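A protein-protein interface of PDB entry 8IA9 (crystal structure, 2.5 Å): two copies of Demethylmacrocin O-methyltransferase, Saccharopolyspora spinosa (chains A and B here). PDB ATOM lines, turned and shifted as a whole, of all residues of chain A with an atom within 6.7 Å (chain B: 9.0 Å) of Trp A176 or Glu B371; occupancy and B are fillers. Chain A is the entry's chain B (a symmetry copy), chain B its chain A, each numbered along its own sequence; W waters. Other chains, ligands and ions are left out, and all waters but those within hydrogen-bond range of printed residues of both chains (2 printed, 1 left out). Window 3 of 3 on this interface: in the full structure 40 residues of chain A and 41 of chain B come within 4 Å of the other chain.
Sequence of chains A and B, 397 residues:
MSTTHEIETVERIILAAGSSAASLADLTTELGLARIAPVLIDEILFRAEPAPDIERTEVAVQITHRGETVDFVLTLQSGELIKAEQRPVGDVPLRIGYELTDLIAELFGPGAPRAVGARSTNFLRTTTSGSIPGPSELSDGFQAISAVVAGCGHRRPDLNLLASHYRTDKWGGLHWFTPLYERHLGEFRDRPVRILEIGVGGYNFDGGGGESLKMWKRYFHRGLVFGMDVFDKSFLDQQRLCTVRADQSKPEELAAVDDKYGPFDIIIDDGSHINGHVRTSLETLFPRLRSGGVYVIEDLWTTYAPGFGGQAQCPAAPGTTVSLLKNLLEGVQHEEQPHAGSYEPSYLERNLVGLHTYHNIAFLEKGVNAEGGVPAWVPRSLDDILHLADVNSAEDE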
ATOM      1  N   ASN A 160       3.319 -14.666 -15.141  1.00  0.00           N
ATOM      2  CA  ASN A 160       1.879 -14.557 -14.774  1.00  0.00           C
ATOM      3  C   ASN A 160       1.663 -15.294 -13.452  1.00  0.00           C
ATOM      4  O   ASN A 160       1.024 -14.718 -12.558  1.00  0.00           O
ATOM      5  CB  ASN A 160       0.923 -15.128 -15.824  1.00  0.00           C
ATOM      6  CG  ASN A 160       0.823 -14.316 -17.101  1.00  0.00           C
ATOM      7  OD1 ASN A 160       1.307 -13.179 -17.186  1.00  0.00           O
ATOM      8  ND2 ASN A 160       0.149 -14.886 -18.091  1.00  0.00           N
ATOM      9  N   ASP A 169      -0.450  -6.888  -7.730  1.00  0.00           N
ATOM     10  CA  ASP A 169      -1.604  -6.412  -8.537  1.00  0.00           C
ATOM     11  C   ASP A 169      -1.185  -6.231 -10.005  1.00  0.00           C
ATOM     12  O   ASP A 169      -2.061  -5.858 -10.819  1.00  0.00           O
ATOM     13  CB  ASP A 169      -2.202  -5.132  -7.939  1.00  0.00           C
ATOM     14  CG  ASP A 169      -1.322  -3.906  -8.102  1.00  0.00           C
ATOM     15  OD1 ASP A 169      -0.337  -4.003  -8.857  1.00  0.00           O
ATOM     16  OD2 ASP A 169      -1.613  -2.874  -7.449  1.00  0.00           O
ATOM     17  N   LYS A 170      -0.003  -6.721 -10.371  1.00  0.00           N
ATOM     18  CA  LYS A 170       0.550  -6.644 -11.752  1.00  0.00           C
ATOM     19  C   LYS A 170      -0.169  -7.625 -12.705  1.00  0.00           C
ATOM     20  O   LYS A 170      -0.231  -7.333 -13.916  1.00  0.00           O
ATOM     21  CB  LYS A 170       2.065  -6.855 -11.684  1.00  0.00           C
ATOM     22  CG  LYS A 170       2.839  -5.568 -11.429  1.00  0.00           C
ATOM     23  CD  LYS A 170       4.264  -5.748 -10.998  1.00  0.00           C
ATOM     24  CE  LYS A 170       5.087  -4.486 -11.172  1.00  0.00           C
ATOM     25  NZ  LYS A 170       4.469  -3.320 -10.499  1.00  0.00           N
ATOM     26  N   TRP A 171      -0.930  -8.572 -12.165  1.00  0.00           N
ATOM     27  CA  TRP A 171      -1.681  -9.584 -12.949  1.00  0.00           C
ATOM     28  C   TRP A 171      -2.883 -10.078 -12.144  1.00  0.00           C
ATOM     29  O   TRP A 171      -2.864  -9.942 -10.905  1.00  0.00           O
ATOM     30  CB  TRP A 171      -0.760 -10.755 -13.331  1.00  0.00           C
ATOM     31  CG  TRP A 171      -1.443 -11.863 -14.074  1.00  0.00           C
ATOM     32  CD1 TRP A 171      -1.912 -13.034 -13.552  1.00  0.00           C
ATOM     33  CD2 TRP A 171      -1.777 -11.885 -15.472  1.00  0.00           C
ATOM     34  NE1 TRP A 171      -2.484 -13.798 -14.539  1.00  0.00           N
ATOM     35  CE2 TRP A 171      -2.408 -13.124 -15.728  1.00  0.00           C
ATOM     36  CE3 TRP A 171      -1.562 -11.009 -16.540  1.00  0.00           C
ATOM     37  CZ2 TRP A 171      -2.868 -13.477 -16.991  1.00  0.00           C
ATOM     38  CZ3 TRP A 171      -2.040 -11.350 -17.786  1.00  0.00           C
ATOM     39  CH2 TRP A 171      -2.725 -12.548 -17.998  1.00  0.00           C
ATOM     40  N   GLY A 172      -3.973 -10.391 -12.835  1.00  0.00           N
ATOM     41  CA  GLY A 172      -5.118 -11.111 -12.250  1.00  0.00           C
ATOM     42  C   GLY A 172      -6.263 -10.224 -11.777  1.00  0.00           C
ATOM     43  O   GLY A 172      -7.073 -10.740 -11.004  1.00  0.00           O
ATOM     44  N   GLY A 173      -6.502  -9.063 -12.386  1.00  0.00           N
ATOM     45  CA  GLY A 173      -7.725  -8.294 -12.081  1.00  0.00           C
ATOM     46  C   GLY A 173      -7.596  -6.815 -12.364  1.00  0.00           C
ATOM     47  O   GLY A 173      -8.277  -6.350 -13.286  1.00  0.00           O
ATOM     48  N   LEU A 174      -6.984  -6.076 -11.442  1.00  0.00           N
ATOM     49  CA  LEU A 174      -6.762  -4.613 -11.573  1.00  0.00           C
ATOM     50  C   LEU A 174      -5.871  -4.330 -12.790  1.00  0.00           C
ATOM     51  O   LEU A 174      -6.144  -3.356 -13.500  1.00  0.00           O
ATOM     52  CB  LEU A 174      -6.151  -4.076 -10.277  1.00  0.00           C
ATOM     53  CG  LEU A 174      -7.163  -3.791  -9.164  1.00  0.00           C
ATOM     54  CD1 LEU A 174      -6.469  -3.578  -7.831  1.00  0.00           C
ATOM     55  CD2 LEU A 174      -8.017  -2.579  -9.503  1.00  0.00           C
ATOM     56  N   HIS A 175      -4.899  -5.196 -13.075  1.00  0.00           N
ATOM     57  CA  HIS A 175      -3.957  -5.023 -14.212  1.00  0.00           C
ATOM     58  C   HIS A 175      -3.684  -6.375 -14.862  1.00  0.00           C
ATOM     59  O   HIS A 175      -3.831  -7.393 -14.160  1.00  0.00           O
ATOM     60  CB  HIS A 175      -2.653  -4.385 -13.729  1.00  0.00           C
ATOM     61  CG  HIS A 175      -2.838  -3.146 -12.921  1.00  0.00           C
ATOM     62  ND1 HIS A 175      -3.455  -2.017 -13.430  1.00  0.00           N
ATOM     63  CD2 HIS A 175      -2.297  -2.778 -11.743  1.00  0.00           C
ATOM     64  CE1 HIS A 175      -3.378  -1.048 -12.545  1.00  0.00           C
ATOM     65  NE2 HIS A 175      -2.643  -1.476 -11.524  1.00  0.00           N
ATOM     66  N   TRP A 176      -3.258  -6.363 -16.129  1.00  0.00           N
ATOM     67  CA  TRP A 176      -2.860  -7.572 -16.908  1.00  0.00           C
ATOM     68  C   TRP A 176      -1.495  -7.320 -17.562  1.00  0.00           C
ATOM     69  O   TRP A 176      -1.381  -7.489 -18.792  1.00  0.00           O
ATOM     70  CB  TRP A 176      -3.943  -7.915 -17.940  1.00  0.00           C
ATOM     71  CG  TRP A 176      -5.297  -8.137 -17.333  1.00  0.00           C
ATOM     72  CD1 TRP A 176      -6.311  -7.230 -17.243  1.00  0.00           C
ATOM     73  CD2 TRP A 176      -5.766  -9.323 -16.666  1.00  0.00           C
ATOM     74  NE1 TRP A 176      -7.369  -7.762 -16.563  1.00  0.00           N
ATOM     75  CE2 TRP A 176      -7.068  -9.045 -16.197  1.00  0.00           C
ATOM     76  CE3 TRP A 176      -5.226 -10.594 -16.433  1.00  0.00           C
ATOM     77  CZ2 TRP A 176      -7.838  -9.993 -15.526  1.00  0.00           C
ATOM     78  CZ3 TRP A 176      -5.999 -11.538 -15.792  1.00  0.00           C
ATOM     79  CH2 TRP A 176      -7.279 -11.233 -15.329  1.00  0.00           C
ATOM     80  N   PHE A 177      -0.509  -6.890 -16.769  1.00  0.00           N
ATOM     81  CA  PHE A 177       0.784  -6.325 -17.258  1.00  0.00           C
ATOM     82  C   PHE A 177       1.813  -7.406 -17.598  1.00  0.00           C
ATOM     83  O   PHE A 177       2.654  -7.117 -18.436  1.00  0.00           O
ATOM     84  CB  PHE A 177       1.421  -5.386 -16.225  1.00  0.00           C
ATOM     85  CG  PHE A 177       0.619  -4.149 -15.933  1.00  0.00           C
ATOM     86  CD1 PHE A 177      -0.209  -3.608 -16.906  1.00  0.00           C
ATOM     87  CD2 PHE A 177       0.864  -3.415 -14.787  1.00  0.00           C
ATOM     88  CE1 PHE A 177      -0.899  -2.433 -16.668  1.00  0.00           C
ATOM     89  CE2 PHE A 177       0.156  -2.249 -14.541  1.00  0.00           C
ATOM     90  CZ  PHE A 177      -0.688  -1.735 -15.498  1.00  0.00           C
ATOM     91  N   THR A 178       1.882  -8.482 -16.819  1.00  0.00           N
ATOM     92  CA  THR A 178       3.064  -9.375 -16.772  1.00  0.00           C
ATOM     93  C   THR A 178       3.400  -9.946 -18.151  1.00  0.00           C
ATOM     94  O   THR A 178       4.560 -10.159 -18.472  1.00  0.00           O
ATOM     95  CB  THR A 178       2.899 -10.430 -15.676  1.00  0.00           C
ATOM     96  OG1 THR A 178       1.603 -11.015 -15.742  1.00  0.00           O
ATOM     97  CG2 THR A 178       3.100  -9.838 -14.302  1.00  0.00           C
ATOM     98  N   PRO A 179       2.438 -10.238 -19.052  1.00  0.00           N
ATOM     99  CA  PRO A 179       2.794 -10.710 -20.393  1.00  0.00           C
ATOM    100  C   PRO A 179       3.542  -9.654 -21.226  1.00  0.00           C
ATOM    101  O   PRO A 179       4.357 -10.023 -22.021  1.00  0.00           O
ATOM    102  CB  PRO A 179       1.430 -11.076 -20.995  1.00  0.00           C
ATOM    103  CG  PRO A 179       0.522 -11.259 -19.818  1.00  0.00           C
ATOM    104  CD  PRO A 179       0.990 -10.207 -18.846  1.00  0.00           C
ATOM    105  N   LEU A 180       3.242  -8.382 -21.003  1.00  0.00           N
ATOM    106  CA  LEU A 180       3.885  -7.266 -21.727  1.00  0.00           C
ATOM    107  C   LEU A 180       5.263  -7.029 -21.121  1.00  0.00           C
ATOM    108  O   LEU A 180       6.143  -6.564 -21.837  1.00  0.00           O
ATOM    109  CB  LEU A 180       2.964  -6.056 -21.588  1.00  0.00           C
ATOM    110  CG  LEU A 180       1.520  -6.269 -22.032  1.00  0.00           C
ATOM    111  CD1 LEU A 180       0.647  -5.108 -21.591  1.00  0.00           C
ATOM    112  CD2 LEU A 180       1.442  -6.464 -23.536  1.00  0.00           C
ATOM    113  N   HIS A 359      -3.035  -0.534 -22.507  1.00  0.00           N
ATOM    114  CA  HIS A 359      -4.012  -0.083 -21.488  1.00  0.00           C
ATOM    115  C   HIS A 359      -3.332   0.039 -20.126  1.00  0.00           C
ATOM    116  O   HIS A 359      -2.828  -0.976 -19.628  1.00  0.00           O
ATOM    117  CB  HIS A 359      -5.198  -1.036 -21.400  1.00  0.00           C
ATOM    118  CG  HIS A 359      -6.188  -0.611 -20.373  1.00  0.00           C
ATOM    119  ND1 HIS A 359      -6.742  -1.503 -19.487  1.00  0.00           N
ATOM    120  CD2 HIS A 359      -6.472   0.614 -19.893  1.00  0.00           C
ATOM    121  CE1 HIS A 359      -7.501  -0.854 -18.638  1.00  0.00           C
ATOM    122  NE2 HIS A 359      -7.303   0.448 -18.825  1.00  0.00           N
ATOM    123  N   ASN A 360      -3.129   1.275 -19.687  1.00  0.00           N
ATOM    124  CA  ASN A 360      -2.711   1.644 -18.313  1.00  0.00           C
ATOM    125  C   ASN A 360      -1.196   1.484 -18.146  1.00  0.00           C
ATOM    126  O   ASN A 360      -0.739   1.439 -17.003  1.00  0.00           O
ATOM    127  CB  ASN A 360      -3.489   0.828 -17.283  1.00  0.00           C
ATOM    128  CG  ASN A 360      -4.143   1.692 -16.228  1.00  0.00           C
ATOM    129  OD1 ASN A 360      -4.059   2.917 -16.292  1.00  0.00           O
ATOM    130  ND2 ASN A 360      -5.013   1.092 -15.433  1.00  0.00           N
ATOM    131  N   VAL B 332      -6.510   4.191 -26.363  1.00  0.00           N
ATOM    132  CA  VAL B 332      -6.249   2.896 -25.681  1.00  0.00           C
ATOM    133  C   VAL B 332      -6.644   3.034 -24.208  1.00  0.00           C
ATOM    134  O   VAL B 332      -7.170   2.057 -23.659  1.00  0.00           O
ATOM    135  CB  VAL B 332      -4.782   2.474 -25.864  1.00  0.00           C
ATOM    136  CG1 VAL B 332      -4.411   1.303 -24.976  1.00  0.00           C
ATOM    137  CG2 VAL B 332      -4.469   2.175 -27.316  1.00  0.00           C
ATOM    138  N   GLN B 333      -6.640   4.262 -23.683  1.00  0.00           N
ATOM    139  CA  GLN B 333      -7.008   4.554 -22.271  1.00  0.00           C
ATOM    140  C   GLN B 333      -8.503   4.891 -22.147  1.00  0.00           C
ATOM    141  O   GLN B 333      -8.901   5.384 -21.082  1.00  0.00           O
ATOM    142  CB  GLN B 333      -6.199   5.742 -21.758  1.00  0.00           C
ATOM    143  CG  GLN B 333      -4.769   5.772 -22.266  1.00  0.00           C
ATOM    144  CD  GLN B 333      -4.045   4.479 -21.995  1.00  0.00           C
ATOM    145  OE1 GLN B 333      -4.232   3.858 -20.953  1.00  0.00           O
ATOM    146  NE2 GLN B 333      -3.188   4.089 -22.929  1.00  0.00           N
ATOM    147  N   HIS B 334      -9.310   4.606 -23.171  1.00  0.00           N
ATOM    148  CA  HIS B 334     -10.690   5.153 -23.300  1.00  0.00           C
ATOM    149  C   HIS B 334     -11.498   4.859 -22.037  1.00  0.00           C
ATOM    150  O   HIS B 334     -12.271   5.732 -21.626  1.00  0.00           O
ATOM    151  CB  HIS B 334     -11.404   4.617 -24.548  1.00  0.00           C
ATOM    152  CG  HIS B 334     -11.752   3.173 -24.458  1.00  0.00           C
ATOM    153  ND1 HIS B 334     -10.921   2.182 -24.957  1.00  0.00           N
ATOM    154  CD2 HIS B 334     -12.871   2.553 -24.017  1.00  0.00           C
ATOM    155  CE1 HIS B 334     -11.526   1.014 -24.853  1.00  0.00           C
ATOM    156  NE2 HIS B 334     -12.718   1.214 -24.269  1.00  0.00           N
ATOM    157  N   GLU B 335     -11.273   3.714 -21.401  1.00  0.00           N
ATOM    158  CA  GLU B 335     -12.063   3.283 -20.218  1.00  0.00           C
ATOM    159  C   GLU B 335     -11.756   4.176 -19.014  1.00  0.00           C
ATOM    160  O   GLU B 335     -12.495   4.073 -18.027  1.00  0.00           O
ATOM    161  CB  GLU B 335     -11.756   1.837 -19.838  1.00  0.00           C
ATOM    162  CG  GLU B 335     -12.285   0.818 -20.817  1.00  0.00           C
ATOM    163  CD  GLU B 335     -11.515  -0.488 -20.773  1.00  0.00           C
ATOM    164  OE1 GLU B 335     -10.250  -0.434 -20.739  1.00  0.00           O
ATOM    165  OE2 GLU B 335     -12.174  -1.542 -20.657  1.00  0.00           O
ATOM    166  N   GLU B 336     -10.663   4.937 -19.047  1.00  0.00           N
ATOM    167  CA  GLU B 336     -10.162   5.699 -17.864  1.00  0.00           C
ATOM    168  C   GLU B 336     -10.511   7.177 -18.025  1.00  0.00           C
ATOM    169  O   GLU B 336     -10.209   7.933 -17.096  1.00  0.00           O
ATOM    170  CB  GLU B 336      -8.649   5.532 -17.686  1.00  0.00           C
ATOM    171  CG  GLU B 336      -8.161   4.095 -17.818  1.00  0.00           C
ATOM    172  CD  GLU B 336      -8.632   3.150 -16.723  1.00  0.00           C
ATOM    173  OE1 GLU B 336      -9.314   3.633 -15.788  1.00  0.00           O
ATOM    174  OE2 GLU B 336      -8.287   1.941 -16.792  1.00  0.00           O
ATOM    175  N   GLU B 349     -10.962   2.582 -30.475  1.00  0.00           N
ATOM    176  CA  GLU B 349     -10.829   2.617 -28.999  1.00  0.00           C
ATOM    177  C   GLU B 349     -10.995   1.190 -28.461  1.00  0.00           C
ATOM    178  O   GLU B 349     -10.113   0.734 -27.718  1.00  0.00           O
ATOM    179  CB  GLU B 349     -11.833   3.607 -28.407  1.00  0.00           C
ATOM    180  CG  GLU B 349     -11.421   5.050 -28.641  1.00  0.00           C
ATOM    181  CD  GLU B 349     -12.438   6.114 -28.264  1.00  0.00           C
ATOM    182  OE1 GLU B 349     -13.625   5.751 -28.042  1.00  0.00           O
ATOM    183  OE2 GLU B 349     -12.044   7.311 -28.216  1.00  0.00           O
ATOM    184  N   ARG B 350     -11.890   0.442 -29.085  1.00  0.00           N
ATOM    185  CA  ARG B 350     -12.366  -0.873 -28.606  1.00  0.00           C
ATOM    186  C   ARG B 350     -11.407  -1.989 -29.057  1.00  0.00           C
ATOM    187  O   ARG B 350     -11.356  -3.012 -28.359  1.00  0.00           O
ATOM    188  CB  ARG B 350     -13.782  -1.051 -29.169  1.00  0.00           C
ATOM    189  CG  ARG B 350     -14.525  -2.295 -28.706  1.00  0.00           C
ATOM    190  CD  ARG B 350     -14.964  -2.238 -27.250  1.00  0.00           C
ATOM    191  NE  ARG B 350     -15.909  -3.296 -26.902  1.00  0.00           N
ATOM    192  CZ  ARG B 350     -15.668  -4.603 -27.023  1.00  0.00           C
ATOM    193  NH1 ARG B 350     -14.538  -5.030 -27.566  1.00  0.00           N
ATOM    194  NH2 ARG B 350     -16.572  -5.484 -26.630  1.00  0.00           N
ATOM    195  N   VAL B 353      -5.211  -2.538 -28.960  1.00  0.00           N
ATOM    196  CA  VAL B 353      -4.747  -3.030 -27.631  1.00  0.00           C
ATOM    197  C   VAL B 353      -3.272  -2.672 -27.428  1.00  0.00           C
ATOM    198  O   VAL B 353      -2.807  -2.761 -26.277  1.00  0.00           O
ATOM    199  CB  VAL B 353      -4.966  -4.546 -27.505  1.00  0.00           C
ATOM    200  CG1 VAL B 353      -6.432  -4.902 -27.627  1.00  0.00           C
ATOM    201  CG2 VAL B 353      -4.129  -5.326 -28.514  1.00  0.00           C
ATOM    202  N   GLY B 354      -2.539  -2.386 -28.508  1.00  0.00           N
ATOM    203  CA  GLY B 354      -1.123  -1.985 -28.441  1.00  0.00           C
ATOM    204  C   GLY B 354      -0.719  -1.097 -29.603  1.00  0.00           C
ATOM    205  O   GLY B 354      -1.092  -1.433 -30.742  1.00  0.00           O
ATOM    206  N   VAL B 368      -9.088  -7.303 -28.465  1.00  0.00           N
ATOM    207  CA  VAL B 368     -10.185  -6.789 -27.605  1.00  0.00           C
ATOM    208  C   VAL B 368      -9.550  -5.917 -26.530  1.00  0.00           C
ATOM    209  O   VAL B 368      -8.904  -6.492 -25.652  1.00  0.00           O
ATOM    210  CB  VAL B 368     -10.975  -7.928 -26.946  1.00  0.00           C
ATOM    211  CG1 VAL B 368     -12.095  -7.376 -26.092  1.00  0.00           C
ATOM    212  CG2 VAL B 368     -11.499  -8.937 -27.955  1.00  0.00           C
ATOM    213  N   ASN B 369      -9.803  -4.610 -26.559  1.00  0.00           N
ATOM    214  CA  ASN B 369      -9.373  -3.653 -25.503  1.00  0.00           C
ATOM    215  C   ASN B 369     -10.570  -3.393 -24.579  1.00  0.00           C
ATOM    216  O   ASN B 369     -11.160  -2.301 -24.658  1.00  0.00           O
ATOM    217  CB  ASN B 369      -8.823  -2.358 -26.103  1.00  0.00           C
ATOM    218  CG  ASN B 369      -8.302  -1.392 -25.059  1.00  0.00           C
ATOM    219  OD1 ASN B 369      -7.944  -1.784 -23.942  1.00  0.00           O
ATOM    220  ND2 ASN B 369      -8.260  -0.119 -25.416  1.00  0.00           N
ATOM    221  N   ALA B 370     -10.806  -4.305 -23.632  1.00  0.00           N
ATOM    222  CA  ALA B 370     -11.958  -4.297 -22.700  1.00  0.00           C
ATOM    223  C   ALA B 370     -11.597  -5.036 -21.407  1.00  0.00           C
ATOM    224  O   ALA B 370     -12.150  -6.126 -21.188  1.00  0.00           O
ATOM    225  CB  ALA B 370     -13.147  -4.947 -23.371  1.00  0.00           C
ATOM    226  N   GLU B 371     -10.604  -4.553 -20.665  1.00  0.00           N
ATOM    227  CA  GLU B 371     -10.199  -5.147 -19.362  1.00  0.00           C
ATOM    228  C   GLU B 371     -10.981  -4.449 -18.243  1.00  0.00           C
ATOM    229  O   GLU B 371     -10.945  -4.929 -17.090  1.00  0.00           O
ATOM    230  CB  GLU B 371      -8.687  -5.004 -19.161  1.00  0.00           C
ATOM    231  CG  GLU B 371      -7.869  -5.581 -20.299  1.00  0.00           C
ATOM    232  CD  GLU B 371      -6.395  -5.226 -20.254  1.00  0.00           C
ATOM    233  OE1 GLU B 371      -6.059  -4.216 -19.592  1.00  0.00           O
ATOM    234  OE2 GLU B 371      -5.589  -5.966 -20.879  1.00  0.00           O
ATOM    235  N   GLY B 372     -11.728  -3.403 -18.596  1.00  0.00           N
ATOM    236  CA  GLY B 372     -12.425  -2.533 -17.631  1.00  0.00           C
ATOM    237  C   GLY B 372     -11.499  -1.449 -17.093  1.00  0.00           C
ATOM    238  O   GLY B 372     -10.265  -1.715 -16.959  1.00  0.00           O
ATOM    239  N   GLY B 373     -12.033  -0.225 -16.993  1.00  0.00           N
ATOM    240  CA  GLY B 373     -11.377   0.958 -16.400  1.00  0.00           C
ATOM    241  C   GLY B 373     -11.220   0.781 -14.904  1.00  0.00           C
ATOM    242  O   GLY B 373     -11.619  -0.283 -14.403  1.00  0.00           O
ATOM    243  N   VAL B 374     -10.454   1.652 -14.251  1.00  0.00           N
ATOM    244  CA  VAL B 374     -10.129   1.482 -12.807  1.00  0.00           C
ATOM    245  C   VAL B 374     -11.437   1.550 -12.029  1.00  0.00           C
ATOM    246  O   VAL B 374     -12.107   2.576 -12.038  1.00  0.00           O
ATOM    247  CB  VAL B 374      -9.114   2.531 -12.318  1.00  0.00           C
ATOM    248  CG1 VAL B 374      -8.814   2.353 -10.840  1.00  0.00           C
ATOM    249  CG2 VAL B 374      -7.832   2.506 -13.131  1.00  0.00           C
ATOM    250  N   PRO B 375     -11.802   0.480 -11.292  1.00  0.00           N
ATOM    251  CA  PRO B 375     -13.050   0.452 -10.529  1.00  0.00           C
ATOM    252  C   PRO B 375     -13.304   1.733  -9.720  1.00  0.00           C
ATOM    253  O   PRO B 375     -12.352   2.343  -9.249  1.00  0.00           O
ATOM    254  CB  PRO B 375     -12.872  -0.734  -9.578  1.00  0.00           C
ATOM    255  CG  PRO B 375     -11.900  -1.639 -10.308  1.00  0.00           C
ATOM    256  CD  PRO B 375     -10.964  -0.703 -11.047  1.00  0.00           C
HETATM  257  O   HOH W   1      -3.567  -2.891 -23.781  1.00  0.00           O
HETATM  258  O   HOH W   2      -3.730  -3.822 -17.959  1.00  0.00           O
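Leu A174 touches Pro B375. Glu B371 touches Trp A176 (CD to CD1, 3.6 Å). Val B332 touches His A359 (CG1 to N, 3.4 Å). His A359 touches Gln B333 (CA to OE1, 3.98 Å). His A359 touches Glu B335. Asn B369 touches His A359. Gly B372 touches His A359. Glu B336 touches Asn A360 (OE2 to ND2, 3.6 Å). CG2 of Val B374 touches ND2 of Asn A360 (3.9 Å).
Of chain B, only Glu B371 comes within 4 Å of Trp A176. Glu B371 touches just these residues of chain A: Trp A176 (3.6 Å) and His A359 (2.8 Å). No residue of chain B comes within 4 Å of Gly A172. Of the printed residues of chain A, Glu B336 touches His A359 (2.7 Å) and Asn A360 (3.6 Å). Of the printed residues of chain A, Asn B369 touches His A359 (3.8 Å). Printed residues of chain A within 4 Å of Gly B372: His A359 (3.3 Å). Of the printed residues of chain A, Val B332 touches His A359. Printed residues of chain B within 4 Å of Asn A360: Gln B333 (3.1 Å), Glu B336 (3.6 Å) and Val B374 (3.9 Å). Asp A169 touches none of the printed residues of chain B. Ala B370 touches none of the printed residues of chain A. The nearest residue of chain B that does not touch Trp A176 is Gly B372 (6.5 Å). The nearest residue of chain A that does not touch Glu B371 is Gly A173 (4.9 Å).
Water W1 lies within hydrogen-bond range of O of Val B353 and N of His A359. Water W2 lies within hydrogen-bond range of OE1 of Glu B371 (2.9 Å), N of Trp A176 (3.2 Å) and O of His A359 (3.4 Å).
OE2 of Glu B336 lies within hydrogen-bond range of NE2 of His A359, 2.7 Å away. The side-chain carboxylate (OE1) of Glu B371 lies within hydrogen-bond range of a ring nitrogen (ND1) of His A359. The side-chain amide oxygen (OE1) of Gln B333 is in hydrogen-bond range of the backbone NH (N) of Asn A360, 3.1 Å away.
No position is printed for both chains. Of the 12 pairs that touch across the chains among the printed residues, none has its exchanged pair printed and touching as well.
The backbone carbonyl oxygen (O) of Val B332 is in hydrogen-bond range of the side-chain amide nitrogen (ND2) of Asn B369, 3.0 Å away. N of Glu B371 sits at hydrogen-bond distance from OE2 of Glu B335 (3.4 Å). The side-chain carboxylate of Glu B335 is in hydrogen-bond range of the backbone NH of Gly B372. The backbone carbonyl oxygen (O) of Glu B349 sits at hydrogen-bond distance from the side-chain amide nitrogen (ND2) of Asn B369, at 3.1 Å. The backbone NH of Asn B369 lies within hydrogen-bond range of the backbone carbonyl oxygen of Arg B350 (2.9 Å). The side-chain carboxylate of Glu B336 is in hydrogen-bond range of the backbone NH of Val B374.
Printed residues of chain B that touch a printed residue of chain A: Val B332, Gln B333, Glu B335, Glu B336, Asn B369, Glu B371, Gly B372, Val B374 and Pro B375. Hydrophobic or aromatic side chains of chain B within 4 Å of the printed part of chain A: Val B332, Val B374 and Pro B375. Of the 15 printed residues of chain A, 4 touch a printed residue of chain B. Hydrophobic or aromatic side chains of chain A within 4 Å of the printed part of chain B: Leu A174, Trp A176 and His A359.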
